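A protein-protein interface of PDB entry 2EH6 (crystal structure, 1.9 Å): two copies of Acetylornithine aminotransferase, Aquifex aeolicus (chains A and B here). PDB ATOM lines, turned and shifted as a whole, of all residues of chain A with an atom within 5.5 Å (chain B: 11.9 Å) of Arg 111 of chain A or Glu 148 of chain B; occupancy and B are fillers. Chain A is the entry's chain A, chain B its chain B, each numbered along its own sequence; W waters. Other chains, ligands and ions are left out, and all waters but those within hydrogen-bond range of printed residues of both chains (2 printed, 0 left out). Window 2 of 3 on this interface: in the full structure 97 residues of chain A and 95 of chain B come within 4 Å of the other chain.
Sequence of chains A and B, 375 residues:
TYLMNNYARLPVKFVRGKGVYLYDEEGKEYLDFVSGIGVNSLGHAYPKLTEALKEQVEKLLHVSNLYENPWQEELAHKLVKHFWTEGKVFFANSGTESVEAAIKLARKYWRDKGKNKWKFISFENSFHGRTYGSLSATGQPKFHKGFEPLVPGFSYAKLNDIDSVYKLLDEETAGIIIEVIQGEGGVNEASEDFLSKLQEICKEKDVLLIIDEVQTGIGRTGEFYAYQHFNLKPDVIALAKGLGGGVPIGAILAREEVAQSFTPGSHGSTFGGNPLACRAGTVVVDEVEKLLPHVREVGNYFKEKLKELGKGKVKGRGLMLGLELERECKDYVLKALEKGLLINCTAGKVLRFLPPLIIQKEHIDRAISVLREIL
NH1 of Arg 111 of chain A lies within salt-bridge range of OE1 of Glu 148 of chain B, 2.7 Å away.
The backbone NH of Lys 108 of chain A sits at hydrogen-bond distance from the backbone carbonyl oxygen of Gly 146 of chain B (3.2 Å).
NH1 of Arg 107 of chain A is in hydrogen-bond range of O of Pro 149 of chain B.
The backbone carbonyl oxygen (O) of Phe 147 of chain B lies within hydrogen-bond range of the guanidinium group (NH1) of Arg 107 of chain A (3.1 Å).
O of Trp 118 of chain A is in hydrogen-bond range of NE of Arg 107 of chain A (2.8 Å).
The side-chain carboxylate (OE1) of Glu 148 of chain B lies within hydrogen-bond range of the backbone NH (N) of Gly 146 of chain B, at 3.1 Å.
O of Phe 147 of chain B is in hydrogen-bond range of OH of Tyr 132 of chain B (2.6 Å).
C of Arg 107 of chain A touches O of Gly 146 of chain B (3.4 Å).
Glu 148 of chain B touches Arg 107 of chain A (C to NH1, 3.6 Å).
Phe 147 of chain B touches Lys 108 of chain A (CE1 to CB, 3.7 Å).
Arg 111 of chain A touches Gly 146 of chain B (NH1 to CA, 3.5 Å).
Pro 149 of chain B touches Trp 118 of chain A (CD to CE3, 3.4 Å).
Arg 107 of chain A touches just these residues of chain B: Tyr 132, Gly 146, Phe 147, Glu 148 and Pro 149.
Lys 108 of chain A touches just these residues of chain B: Gly 146 and Phe 147.
No residue of chain B comes within 4 Å of Asp 112 of chain A.
No residue of chain B comes within 4 Å of Gly 114 of chain A.
Of the printed residues of chain A, Tyr 132 of chain B touches Arg 107 (3.4 Å).
Printed residues of chain A within 4 Å of Gly 146 of chain B: Arg 107 (3.4 Å), Lys 108 (3.2 Å) and Arg 111 (3.5 Å).
Printed residues of chain A within 4 Å of Glu 148 of chain B: Arg 107 (3.6 Å) and Arg 111 (2.7 Å).
The nearest printed residue of chain A that does not touch Gly 146 of chain B is Tyr 109 of chain A (5.6 Å).
Printed residues of chain B that touch a printed residue of chain A: Tyr 132, Gly 146, Phe 147, Glu 148 and Pro 149.
Hydrophobic or aromatic side chains of chain B that line the printed part of chain A: Tyr 132, Phe 147 and Pro 149.
Of the 11 printed residues of chain A, 4 touch a printed residue of chain B.
Hydrophobic or aromatic side chains of chain A within 4 Å of the printed part of chain B: Trp 118.
Among the printed residues, Asp or Glu carboxylates within 4 Å of a Lys or Arg side-chain nitrogen of the other chain: Arg 111 of chain A with Glu 148 of chain B.
No position is printed for both chains.
Water W1 lies within hydrogen-bond range of the side-chain amino group of Lys 145 of chain B and the side-chain carboxylate of Asp 112 of chain A.
Water W2 bridges O of Glu 148 of chain B (2.7 Å) and NH1 of Arg 111 of chain A (2.8 Å).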
ATOM      1  N   ALA A 106      21.919  22.638 -14.147  1.00  0.00           N
ATOM      2  CA  ALA A 106      22.462  22.236 -15.436  1.00  0.00           C
ATOM      3  C   ALA A 106      23.164  20.883 -15.348  1.00  0.00           C
ATOM      4  O   ALA A 106      22.997  20.037 -16.227  1.00  0.00           O
ATOM      5  CB  ALA A 106      23.427  23.291 -15.941  1.00  0.00           C
ATOM      6  N   ARG A 107      23.958  20.685 -14.298  1.00  0.00           N
ATOM      7  CA  ARG A 107      24.658  19.417 -14.123  1.00  0.00           C
ATOM      8  C   ARG A 107      23.686  18.277 -13.866  1.00  0.00           C
ATOM      9  O   ARG A 107      23.790  17.219 -14.490  1.00  0.00           O
ATOM     10  CB  ARG A 107      25.674  19.497 -12.979  1.00  0.00           C
ATOM     11  CG  ARG A 107      26.993  20.116 -13.399  1.00  0.00           C
ATOM     12  CD  ARG A 107      28.065  19.985 -12.338  1.00  0.00           C
ATOM     13  NE  ARG A 107      29.353  20.454 -12.851  1.00  0.00           N
ATOM     14  CZ  ARG A 107      30.455  20.581 -12.120  1.00  0.00           C
ATOM     15  NH1 ARG A 107      30.441  20.272 -10.827  1.00  0.00           N
ATOM     16  NH2 ARG A 107      31.573  21.025 -12.680  1.00  0.00           N
ATOM     17  N   LYS A 108      22.734  18.485 -12.960  1.00  0.00           N
ATOM     18  CA  LYS A 108      21.773  17.433 -12.661  1.00  0.00           C
ATOM     19  C   LYS A 108      20.893  17.130 -13.871  1.00  0.00           C
ATOM     20  O   LYS A 108      20.499  15.980 -14.092  1.00  0.00           O
ATOM     21  CB  LYS A 108      20.900  17.809 -11.463  1.00  0.00           C
ATOM     22  CG  LYS A 108      19.980  16.683 -11.045  1.00  0.00           C
ATOM     23  CD  LYS A 108      19.426  16.872  -9.656  1.00  0.00           C
ATOM     24  CE  LYS A 108      18.562  15.688  -9.265  1.00  0.00           C
ATOM     25  NZ  LYS A 108      17.420  15.514 -10.216  1.00  0.00           N
ATOM     26  N   TYR A 109      20.604  18.160 -14.660  1.00  0.00           N
ATOM     27  CA  TYR A 109      19.785  17.999 -15.856  1.00  0.00           C
ATOM     28  C   TYR A 109      20.333  16.880 -16.745  1.00  0.00           C
ATOM     29  O   TYR A 109      19.605  15.956 -17.118  1.00  0.00           O
ATOM     30  CB  TYR A 109      19.762  19.303 -16.651  1.00  0.00           C
ATOM     31  CG  TYR A 109      19.081  19.189 -17.996  1.00  0.00           C
ATOM     32  CD1 TYR A 109      17.711  18.959 -18.088  1.00  0.00           C
ATOM     33  CD2 TYR A 109      19.807  19.320 -19.178  1.00  0.00           C
ATOM     34  CE1 TYR A 109      17.076  18.867 -19.326  1.00  0.00           C
ATOM     35  CE2 TYR A 109      19.184  19.227 -20.424  1.00  0.00           C
ATOM     36  CZ  TYR A 109      17.820  19.003 -20.488  1.00  0.00           C
ATOM     37  OH  TYR A 109      17.199  18.913 -21.714  1.00  0.00           O
ATOM     38  N   TRP A 110      21.619  16.974 -17.076  1.00  0.00           N
ATOM     39  CA  TRP A 110      22.268  15.985 -17.929  1.00  0.00           C
ATOM     40  C   TRP A 110      22.406  14.628 -17.254  1.00  0.00           C
ATOM     41  O   TRP A 110      22.397  13.597 -17.926  1.00  0.00           O
ATOM     42  CB  TRP A 110      23.636  16.498 -18.387  1.00  0.00           C
ATOM     43  CG  TRP A 110      23.537  17.667 -19.319  1.00  0.00           C
ATOM     44  CD1 TRP A 110      24.015  18.929 -19.107  1.00  0.00           C
ATOM     45  CD2 TRP A 110      22.906  17.689 -20.606  1.00  0.00           C
ATOM     46  NE1 TRP A 110      23.722  19.734 -20.182  1.00  0.00           N
ATOM     47  CE2 TRP A 110      23.042  18.998 -21.116  1.00  0.00           C
ATOM     48  CE3 TRP A 110      22.239  16.726 -21.380  1.00  0.00           C
ATOM     49  CZ2 TRP A 110      22.535  19.372 -22.367  1.00  0.00           C
ATOM     50  CZ3 TRP A 110      21.733  17.100 -22.625  1.00  0.00           C
ATOM     51  CH2 TRP A 110      21.887  18.412 -23.105  1.00  0.00           C
ATOM     52  N   ARG A 111      22.534  14.623 -15.932  1.00  0.00           N
ATOM     53  CA  ARG A 111      22.635  13.372 -15.190  1.00  0.00           C
ATOM     54  C   ARG A 111      21.302  12.636 -15.256  1.00  0.00           C
ATOM     55  O   ARG A 111      21.265  11.409 -15.401  1.00  0.00           O
ATOM     56  CB  ARG A 111      23.003  13.635 -13.726  1.00  0.00           C
ATOM     57  CG  ARG A 111      24.467  13.972 -13.504  1.00  0.00           C
ATOM     58  CD  ARG A 111      25.337  12.723 -13.559  1.00  0.00           C
ATOM     59  NE  ARG A 111      25.220  11.909 -12.348  1.00  0.00           N
ATOM     60  CZ  ARG A 111      25.833  12.178 -11.197  1.00  0.00           C
ATOM     61  NH1 ARG A 111      26.615  13.243 -11.087  1.00  0.00           N
ATOM     62  NH2 ARG A 111      25.668  11.377 -10.151  1.00  0.00           N
ATOM     63  N   ASP A 112      20.204  13.377 -15.151  1.00  0.00           N
ATOM     64  CA  ASP A 112      18.885  12.754 -15.238  1.00  0.00           C
ATOM     65  C   ASP A 112      18.654  12.117 -16.610  1.00  0.00           C
ATOM     66  O   ASP A 112      17.870  11.190 -16.780  1.00  0.00           O
ATOM     67  CB  ASP A 112      17.820  13.830 -14.996  1.00  0.00           C
ATOM     68  CG  ASP A 112      17.875  14.316 -13.553  1.00  0.00           C
ATOM     69  OD1 ASP A 112      18.177  13.503 -12.680  1.00  0.00           O
ATOM     70  OD2 ASP A 112      17.576  15.485 -13.314  1.00  0.00           O
ATOM     71  N   LYS A 113      19.344  12.686 -17.619  1.00  0.00           N
ATOM     72  CA  LYS A 113      19.163  12.216 -18.993  1.00  0.00           C
ATOM     73  C   LYS A 113      20.138  11.096 -19.357  1.00  0.00           C
ATOM     74  O   LYS A 113      20.195  10.625 -20.485  1.00  0.00           O
ATOM     75  CB  LYS A 113      19.383  13.403 -19.926  1.00  0.00           C
ATOM     76  CG  LYS A 113      18.233  14.411 -19.870  1.00  0.00           C
ATOM     77  CD  LYS A 113      18.080  15.184 -21.182  1.00  0.00           C
ATOM     78  CE  LYS A 113      16.816  16.047 -21.205  1.00  0.00           C
ATOM     79  NZ  LYS A 113      15.666  15.237 -20.812  1.00  0.00           N
ATOM     80  N   GLY A 114      20.966  10.709 -18.366  1.00  0.00           N
ATOM     81  CA  GLY A 114      21.883   9.592 -18.584  1.00  0.00           C
ATOM     82  C   GLY A 114      23.201  10.024 -19.241  1.00  0.00           C
ATOM     83  O   GLY A 114      24.008   9.208 -19.668  1.00  0.00           O
ATOM     84  N   LYS A 115      23.408  11.351 -19.324  1.00  0.00           N
ATOM     85  CA  LYS A 115      24.584  11.837 -20.043  1.00  0.00           C
ATOM     86  C   LYS A 115      25.681  12.357 -19.110  1.00  0.00           C
ATOM     87  O   LYS A 115      25.435  12.740 -17.974  1.00  0.00           O
ATOM     88  CB  LYS A 115      24.135  12.940 -21.003  1.00  0.00           C
ATOM     89  CG  LYS A 115      23.179  12.414 -22.075  1.00  0.00           C
ATOM     90  CD  LYS A 115      22.844  13.470 -23.130  1.00  0.00           C
ATOM     91  CE  LYS A 115      21.887  12.938 -24.203  1.00  0.00           C
ATOM     92  NZ  LYS A 115      21.581  13.999 -25.161  1.00  0.00           N
ATOM     93  N   TRP A 118      29.386  17.789 -17.561  1.00  0.00           N
ATOM     94  CA  TRP A 118      29.524  18.488 -16.295  1.00  0.00           C
ATOM     95  C   TRP A 118      30.422  19.717 -16.356  1.00  0.00           C
ATOM     96  O   TRP A 118      30.603  20.404 -15.349  1.00  0.00           O
ATOM     97  CB  TRP A 118      30.044  17.530 -15.214  1.00  0.00           C
ATOM     98  CG  TRP A 118      31.315  16.863 -15.655  1.00  0.00           C
ATOM     99  CD1 TRP A 118      31.426  15.766 -16.461  1.00  0.00           C
ATOM    100  CD2 TRP A 118      32.653  17.311 -15.402  1.00  0.00           C
ATOM    101  NE1 TRP A 118      32.748  15.505 -16.730  1.00  0.00           N
ATOM    102  CE2 TRP A 118      33.523  16.437 -16.092  1.00  0.00           C
ATOM    103  CE3 TRP A 118      33.200  18.367 -14.663  1.00  0.00           C
ATOM    104  CZ2 TRP A 118      34.914  16.589 -16.064  1.00  0.00           C
ATOM    105  CZ3 TRP A 118      34.585  18.516 -14.635  1.00  0.00           C
ATOM    106  CH2 TRP A 118      35.424  17.630 -15.332  1.00  0.00           C
ATOM    107  N   ARG B 130      23.871  24.570   0.539  1.00  0.00           N
ATOM    108  CA  ARG B 130      23.632  23.978  -0.771  1.00  0.00           C
ATOM    109  C   ARG B 130      24.507  24.515  -1.900  1.00  0.00           C
ATOM    110  O   ARG B 130      24.517  23.944  -2.991  1.00  0.00           O
ATOM    111  CB  ARG B 130      22.164  24.163  -1.154  1.00  0.00           C
ATOM    112  CG  ARG B 130      21.169  23.541  -0.189  1.00  0.00           C
ATOM    113  CD  ARG B 130      21.058  22.040  -0.375  1.00  0.00           C
ATOM    114  NE  ARG B 130      19.755  21.558   0.077  1.00  0.00           N
ATOM    115  CZ  ARG B 130      19.211  20.402  -0.295  1.00  0.00           C
ATOM    116  NH1 ARG B 130      19.860  19.599  -1.127  1.00  0.00           N
ATOM    117  NH2 ARG B 130      18.009  20.059   0.148  1.00  0.00           N
ATOM    118  N   THR B 131      25.207  25.623  -1.664  1.00  0.00           N
ATOM    119  CA  THR B 131      26.089  26.175  -2.688  1.00  0.00           C
ATOM    120  C   THR B 131      27.329  25.275  -2.705  1.00  0.00           C
ATOM    121  O   THR B 131      27.626  24.620  -1.708  1.00  0.00           O
ATOM    122  CB  THR B 131      26.447  27.657  -2.394  1.00  0.00           C
ATOM    123  OG1 THR B 131      26.848  27.805  -1.026  1.00  0.00           O
ATOM    124  CG2 THR B 131      25.227  28.546  -2.661  1.00  0.00           C
ATOM    125  N   TYR B 132      28.042  25.232  -3.825  1.00  0.00           N
ATOM    126  CA  TYR B 132      29.184  24.323  -3.966  1.00  0.00           C
ATOM    127  C   TYR B 132      30.186  24.158  -2.833  1.00  0.00           C
ATOM    128  O   TYR B 132      30.533  23.025  -2.490  1.00  0.00           O
ATOM    129  CB  TYR B 132      29.907  24.592  -5.289  1.00  0.00           C
ATOM    130  CG  TYR B 132      29.313  23.757  -6.402  1.00  0.00           C
ATOM    131  CD1 TYR B 132      29.655  22.407  -6.540  1.00  0.00           C
ATOM    132  CD2 TYR B 132      28.330  24.277  -7.249  1.00  0.00           C
ATOM    133  CE1 TYR B 132      29.028  21.591  -7.485  1.00  0.00           C
ATOM    134  CE2 TYR B 132      27.693  23.467  -8.203  1.00  0.00           C
ATOM    135  CZ  TYR B 132      28.048  22.124  -8.310  1.00  0.00           C
ATOM    136  OH  TYR B 132      27.414  21.312  -9.227  1.00  0.00           O
ATOM    137  N   GLY B 133      30.653  25.251  -2.241  1.00  0.00           N
ATOM    138  CA  GLY B 133      31.605  25.119  -1.149  1.00  0.00           C
ATOM    139  C   GLY B 133      30.961  24.462   0.058  1.00  0.00           C
ATOM    140  O   GLY B 133      31.487  23.495   0.623  1.00  0.00           O
ATOM    141  N   LEU B 135      28.216  22.767   0.091  1.00  0.00           N
ATOM    142  CA  LEU B 135      27.717  21.445  -0.273  1.00  0.00           C
ATOM    143  C   LEU B 135      28.826  20.396  -0.152  1.00  0.00           C
ATOM    144  O   LEU B 135      28.567  19.249   0.209  1.00  0.00           O
ATOM    145  CB  LEU B 135      27.174  21.467  -1.700  1.00  0.00           C
ATOM    146  CG  LEU B 135      26.539  20.172  -2.218  1.00  0.00           C
ATOM    147  CD1 LEU B 135      25.340  19.800  -1.358  1.00  0.00           C
ATOM    148  CD2 LEU B 135      26.123  20.367  -3.669  1.00  0.00           C
ATOM    149  N   SER B 136      30.054  20.801  -0.455  1.00  0.00           N
ATOM    150  CA  SER B 136      31.198  19.902  -0.379  1.00  0.00           C
ATOM    151  C   SER B 136      31.502  19.575   1.073  1.00  0.00           C
ATOM    152  O   SER B 136      31.998  18.493   1.390  1.00  0.00           O
ATOM    153  CB  SER B 136      32.420  20.546  -1.031  1.00  0.00           C
ATOM    154  OG  SER B 136      32.138  20.922  -2.367  1.00  0.00           O
ATOM    155  N   ALA B 137      31.200  20.522   1.953  1.00  0.00           N
ATOM    156  CA  ALA B 137      31.428  20.353   3.376  1.00  0.00           C
ATOM    157  C   ALA B 137      30.314  19.523   3.996  1.00  0.00           C
ATOM    158  O   ALA B 137      30.510  18.871   5.013  1.00  0.00           O
ATOM    159  CB  ALA B 137      31.504  21.723   4.055  1.00  0.00           C
ATOM    160  N   THR B 138      29.140  19.559   3.373  1.00  0.00           N
ATOM    161  CA  THR B 138      27.980  18.821   3.850  1.00  0.00           C
ATOM    162  C   THR B 138      28.246  17.318   3.694  1.00  0.00           C
ATOM    163  O   THR B 138      28.432  16.819   2.583  1.00  0.00           O
ATOM    164  CB  THR B 138      26.720  19.266   3.065  1.00  0.00           C
ATOM    165  OG1 THR B 138      26.440  20.642   3.373  1.00  0.00           O
ATOM    166  CG2 THR B 138      25.513  18.419   3.428  1.00  0.00           C
ATOM    167  N   GLY B 139      28.276  16.608   4.819  1.00  0.00           N
ATOM    168  CA  GLY B 139      28.571  15.185   4.795  1.00  0.00           C
ATOM    169  C   GLY B 139      27.397  14.264   4.543  1.00  0.00           C
ATOM    170  O   GLY B 139      27.166  13.324   5.303  1.00  0.00           O
ATOM    171  N   GLN B 140      26.653  14.534   3.479  1.00  0.00           N
ATOM    172  CA  GLN B 140      25.504  13.722   3.115  1.00  0.00           C
ATOM    173  C   GLN B 140      25.465  13.577   1.599  1.00  0.00           C
ATOM    174  O   GLN B 140      24.922  14.429   0.894  1.00  0.00           O
ATOM    175  CB  GLN B 140      24.214  14.367   3.622  1.00  0.00           C
ATOM    176  CG  GLN B 140      24.149  14.481   5.133  1.00  0.00           C
ATOM    177  CD  GLN B 140      22.784  14.912   5.619  1.00  0.00           C
ATOM    178  OE1 GLN B 140      21.794  14.209   5.416  1.00  0.00           O
ATOM    179  NE2 GLN B 140      22.720  16.075   6.266  1.00  0.00           N
ATOM    180  N   PRO B 141      26.049  12.484   1.081  1.00  0.00           N
ATOM    181  CA  PRO B 141      26.103  12.199  -0.353  1.00  0.00           C
ATOM    182  C   PRO B 141      24.774  12.348  -1.090  1.00  0.00           C
ATOM    183  O   PRO B 141      24.755  12.723  -2.262  1.00  0.00           O
ATOM    184  CB  PRO B 141      26.633  10.767  -0.398  1.00  0.00           C
ATOM    185  CG  PRO B 141      27.529  10.710   0.796  1.00  0.00           C
ATOM    186  CD  PRO B 141      26.688  11.402   1.852  1.00  0.00           C
ATOM    187  N   LYS B 142      23.666  12.061  -0.415  1.00  0.00           N
ATOM    188  CA  LYS B 142      22.369  12.172  -1.071  1.00  0.00           C
ATOM    189  C   LYS B 142      22.133  13.578  -1.606  1.00  0.00           C
ATOM    190  O   LYS B 142      21.438  13.752  -2.604  1.00  0.00           O
ATOM    191  CB  LYS B 142      21.235  11.766  -0.125  1.00  0.00           C
ATOM    192  CG  LYS B 142      20.961  12.719   1.024  1.00  0.00           C
ATOM    193  CD  LYS B 142      19.818  12.181   1.869  1.00  0.00           C
ATOM    194  CE  LYS B 142      19.554  13.036   3.095  1.00  0.00           C
ATOM    195  NZ  LYS B 142      18.506  12.407   3.950  1.00  0.00           N
ATOM    196  N   PHE B 143      22.722  14.578  -0.951  1.00  0.00           N
ATOM    197  CA  PHE B 143      22.552  15.963  -1.393  1.00  0.00           C
ATOM    198  C   PHE B 143      23.566  16.325  -2.494  1.00  0.00           C
ATOM    199  O   PHE B 143      23.480  17.355  -3.148  1.00  0.00           O
ATOM    200  CB  PHE B 143      22.737  16.918  -0.198  1.00  0.00           C
ATOM    201  CG  PHE B 143      21.652  16.763   0.839  1.00  0.00           C
ATOM    202  CD1 PHE B 143      20.314  16.702   0.457  1.00  0.00           C
ATOM    203  CD2 PHE B 143      21.985  16.753   2.183  1.00  0.00           C
ATOM    204  CE1 PHE B 143      19.318  16.612   1.427  1.00  0.00           C
ATOM    205  CE2 PHE B 143      20.990  16.661   3.150  1.00  0.00           C
ATOM    206  CZ  PHE B 143      19.655  16.581   2.777  1.00  0.00           C
ATOM    207  N   HIS B 144      24.592  15.451  -2.652  1.00  0.00           N
ATOM    208  CA  HIS B 144      25.598  15.681  -3.698  1.00  0.00           C
ATOM    209  C   HIS B 144      25.134  15.106  -5.048  1.00  0.00           C
ATOM    210  O   HIS B 144      25.608  15.472  -6.120  1.00  0.00           O
ATOM    211  CB  HIS B 144      26.910  14.976  -3.302  1.00  0.00           C
ATOM    212  CG  HIS B 144      27.477  15.444  -1.981  1.00  0.00           C
ATOM    213  ND1 HIS B 144      28.458  14.774  -1.335  1.00  0.00           N
ATOM    214  CD2 HIS B 144      27.173  16.595  -1.236  1.00  0.00           C
ATOM    215  CE1 HIS B 144      28.739  15.487  -0.228  1.00  0.00           C
ATOM    216  NE2 HIS B 144      27.984  16.584  -0.141  1.00  0.00           N
ATOM    217  N   LYS B 145      24.208  14.119  -4.945  1.00  0.00           N
ATOM    218  CA  LYS B 145      23.733  13.329  -6.087  1.00  0.00           C
ATOM    219  C   LYS B 145      23.290  14.176  -7.305  1.00  0.00           C
ATOM    220  O   LYS B 145      22.238  14.799  -7.321  1.00  0.00           O
ATOM    221  CB  LYS B 145      22.565  12.481  -5.560  1.00  0.00           C
ATOM    222  CG  LYS B 145      22.128  11.360  -6.516  1.00  0.00           C
ATOM    223  CD  LYS B 145      21.079  11.820  -7.538  1.00  0.00           C
ATOM    224  CE  LYS B 145      20.608  10.684  -8.449  1.00  0.00           C
ATOM    225  NZ  LYS B 145      19.404  11.110  -9.168  1.00  0.00           N
ATOM    226  N   GLY B 146      24.139  14.148  -8.334  1.00  0.00           N
ATOM    227  CA  GLY B 146      23.841  14.842  -9.574  1.00  0.00           C
ATOM    228  C   GLY B 146      24.569  16.151  -9.806  1.00  0.00           C
ATOM    229  O   GLY B 146      24.469  16.728 -10.888  1.00  0.00           O
ATOM    230  N   PHE B 147      25.325  16.607  -8.810  1.00  0.00           N
ATOM    231  CA  PHE B 147      26.033  17.880  -8.912  1.00  0.00           C
ATOM    232  C   PHE B 147      27.549  17.780  -9.006  1.00  0.00           C
ATOM    233  O   PHE B 147      28.233  18.792  -9.208  1.00  0.00           O
ATOM    234  CB  PHE B 147      25.640  18.749  -7.712  1.00  0.00           C
ATOM    235  CG  PHE B 147      24.165  18.822  -7.496  1.00  0.00           C
ATOM    236  CD1 PHE B 147      23.339  19.391  -8.457  1.00  0.00           C
ATOM    237  CD2 PHE B 147      23.591  18.290  -6.347  1.00  0.00           C
ATOM    238  CE1 PHE B 147      21.954  19.425  -8.280  1.00  0.00           C
ATOM    239  CE2 PHE B 147      22.211  18.319  -6.161  1.00  0.00           C
ATOM    240  CZ  PHE B 147      21.392  18.888  -7.133  1.00  0.00           C
ATOM    241  N   GLU B 148      28.072  16.567  -8.854  1.00  0.00           N
ATOM    242  CA  GLU B 148      29.508  16.328  -8.909  1.00  0.00           C
ATOM    243  C   GLU B 148      30.082  16.753 -10.254  1.00  0.00           C
ATOM    244  O   GLU B 148      29.378  16.766 -11.257  1.00  0.00           O
ATOM    245  CB  GLU B 148      29.809  14.844  -8.660  1.00  0.00           C
ATOM    246  CG  GLU B 148      29.252  14.308  -7.349  1.00  0.00           C
ATOM    247  CD  GLU B 148      27.906  13.611  -7.509  1.00  0.00           C
ATOM    248  OE1 GLU B 148      27.219  13.822  -8.533  1.00  0.00           O
ATOM    249  OE2 GLU B 148      27.530  12.856  -6.592  1.00  0.00           O
ATOM    250  N   PRO B 149      31.380  17.098 -10.294  1.00  0.00           N
ATOM    251  CA  PRO B 149      32.335  17.117  -9.182  1.00  0.00           C
ATOM    252  C   PRO B 149      32.185  18.311  -8.237  1.00  0.00           C
ATOM    253  O   PRO B 149      31.883  19.424  -8.666  1.00  0.00           O
ATOM    254  CB  PRO B 149      33.679  17.129  -9.895  1.00  0.00           C
ATOM    255  CG  PRO B 149      33.388  17.966 -11.090  1.00  0.00           C
ATOM    256  CD  PRO B 149      32.050  17.446 -11.559  1.00  0.00           C
ATOM    257  N   LEU B 150      32.415  18.063  -6.951  1.00  0.00           N
ATOM    258  CA  LEU B 150      32.330  19.104  -5.930  1.00  0.00           C
ATOM    259  C   LEU B 150      33.700  19.753  -5.768  1.00  0.00           C
ATOM    260  O   LEU B 150      34.623  19.461  -6.531  1.00  0.00           O
ATOM    261  CB  LEU B 150      31.898  18.486  -4.601  1.00  0.00           C
ATOM    262  CG  LEU B 150      30.629  17.635  -4.666  1.00  0.00           C
ATOM    263  CD1 LEU B 150      30.413  16.913  -3.350  1.00  0.00           C
ATOM    264  CD2 LEU B 150      29.447  18.521  -5.005  1.00  0.00           C
ATOM    265  N   VAL B 151      33.832  20.643  -4.786  1.00  0.00           N
ATOM    266  CA  VAL B 151      35.118  21.281  -4.536  1.00  0.00           C
ATOM    267  C   VAL B 151      36.018  20.213  -3.916  1.00  0.00           C
ATOM    268  O   VAL B 151      35.642  19.565  -2.937  1.00  0.00           O
ATOM    269  CB  VAL B 151      35.011  22.454  -3.546  1.00  0.00           C
ATOM    270  CG1 VAL B 151      36.369  23.137  -3.421  1.00  0.00           C
ATOM    271  CG2 VAL B 151      33.957  23.452  -4.014  1.00  0.00           C
ATOM    272  N   PRO B 152      37.218  20.016  -4.475  1.00  0.00           N
ATOM    273  CA  PRO B 152      38.157  19.010  -3.962  1.00  0.00           C
ATOM    274  C   PRO B 152      38.705  19.341  -2.576  1.00  0.00           C
ATOM    275  O   PRO B 152      38.813  20.512  -2.212  1.00  0.00           O
ATOM    276  CB  PRO B 152      39.272  19.005  -5.013  1.00  0.00           C
ATOM    277  CG  PRO B 152      38.606  19.535  -6.258  1.00  0.00           C
ATOM    278  CD  PRO B 152      37.740  20.640  -5.704  1.00  0.00           C
ATOM    279  N   PHE B 154      37.538  17.817   0.564  1.00  0.00           N
ATOM    280  CA  PHE B 154      36.684  17.536   1.711  1.00  0.00           C
ATOM    281  C   PHE B 154      36.506  16.051   2.007  1.00  0.00           C
ATOM    282  O   PHE B 154      36.152  15.275   1.124  1.00  0.00           O
ATOM    283  CB  PHE B 154      35.301  18.170   1.515  1.00  0.00           C
ATOM    284  CG  PHE B 154      35.323  19.672   1.456  1.00  0.00           C
ATOM    285  CD1 PHE B 154      35.782  20.331   0.317  1.00  0.00           C
ATOM    286  CD2 PHE B 154      34.909  20.428   2.547  1.00  0.00           C
ATOM    287  CE1 PHE B 154      35.827  21.723   0.268  1.00  0.00           C
ATOM    288  CE2 PHE B 154      34.953  21.820   2.511  1.00  0.00           C
ATOM    289  CZ  PHE B 154      35.413  22.468   1.369  1.00  0.00           C
ATOM    290  N   TYR B 156      34.950  13.216   5.154  1.00  0.00           N
ATOM    291  CA  TYR B 156      33.989  13.157   6.245  1.00  0.00           C
ATOM    292  C   TYR B 156      34.293  12.183   7.378  1.00  0.00           C
ATOM    293  O   TYR B 156      34.285  10.969   7.184  1.00  0.00           O
ATOM    294  CB  TYR B 156      32.616  12.839   5.654  1.00  0.00           C
ATOM    295  CG  TYR B 156      32.317  13.645   4.407  1.00  0.00           C
ATOM    296  CD1 TYR B 156      32.284  15.046   4.446  1.00  0.00           C
ATOM    297  CD2 TYR B 156      32.088  13.015   3.182  1.00  0.00           C
ATOM    298  CE1 TYR B 156      32.035  15.796   3.292  1.00  0.00           C
ATOM    299  CE2 TYR B 156      31.836  13.756   2.022  1.00  0.00           C
ATOM    300  CZ  TYR B 156      31.812  15.144   2.087  1.00  0.00           C
ATOM    301  OH  TYR B 156      31.575  15.874   0.944  1.00  0.00           O
HETATM  302  O   HOH W   1      20.498  12.767 -10.955  1.00  0.00           O
HETATM  303  O   HOH W   2      27.635  15.285 -12.745  1.00  0.00           O
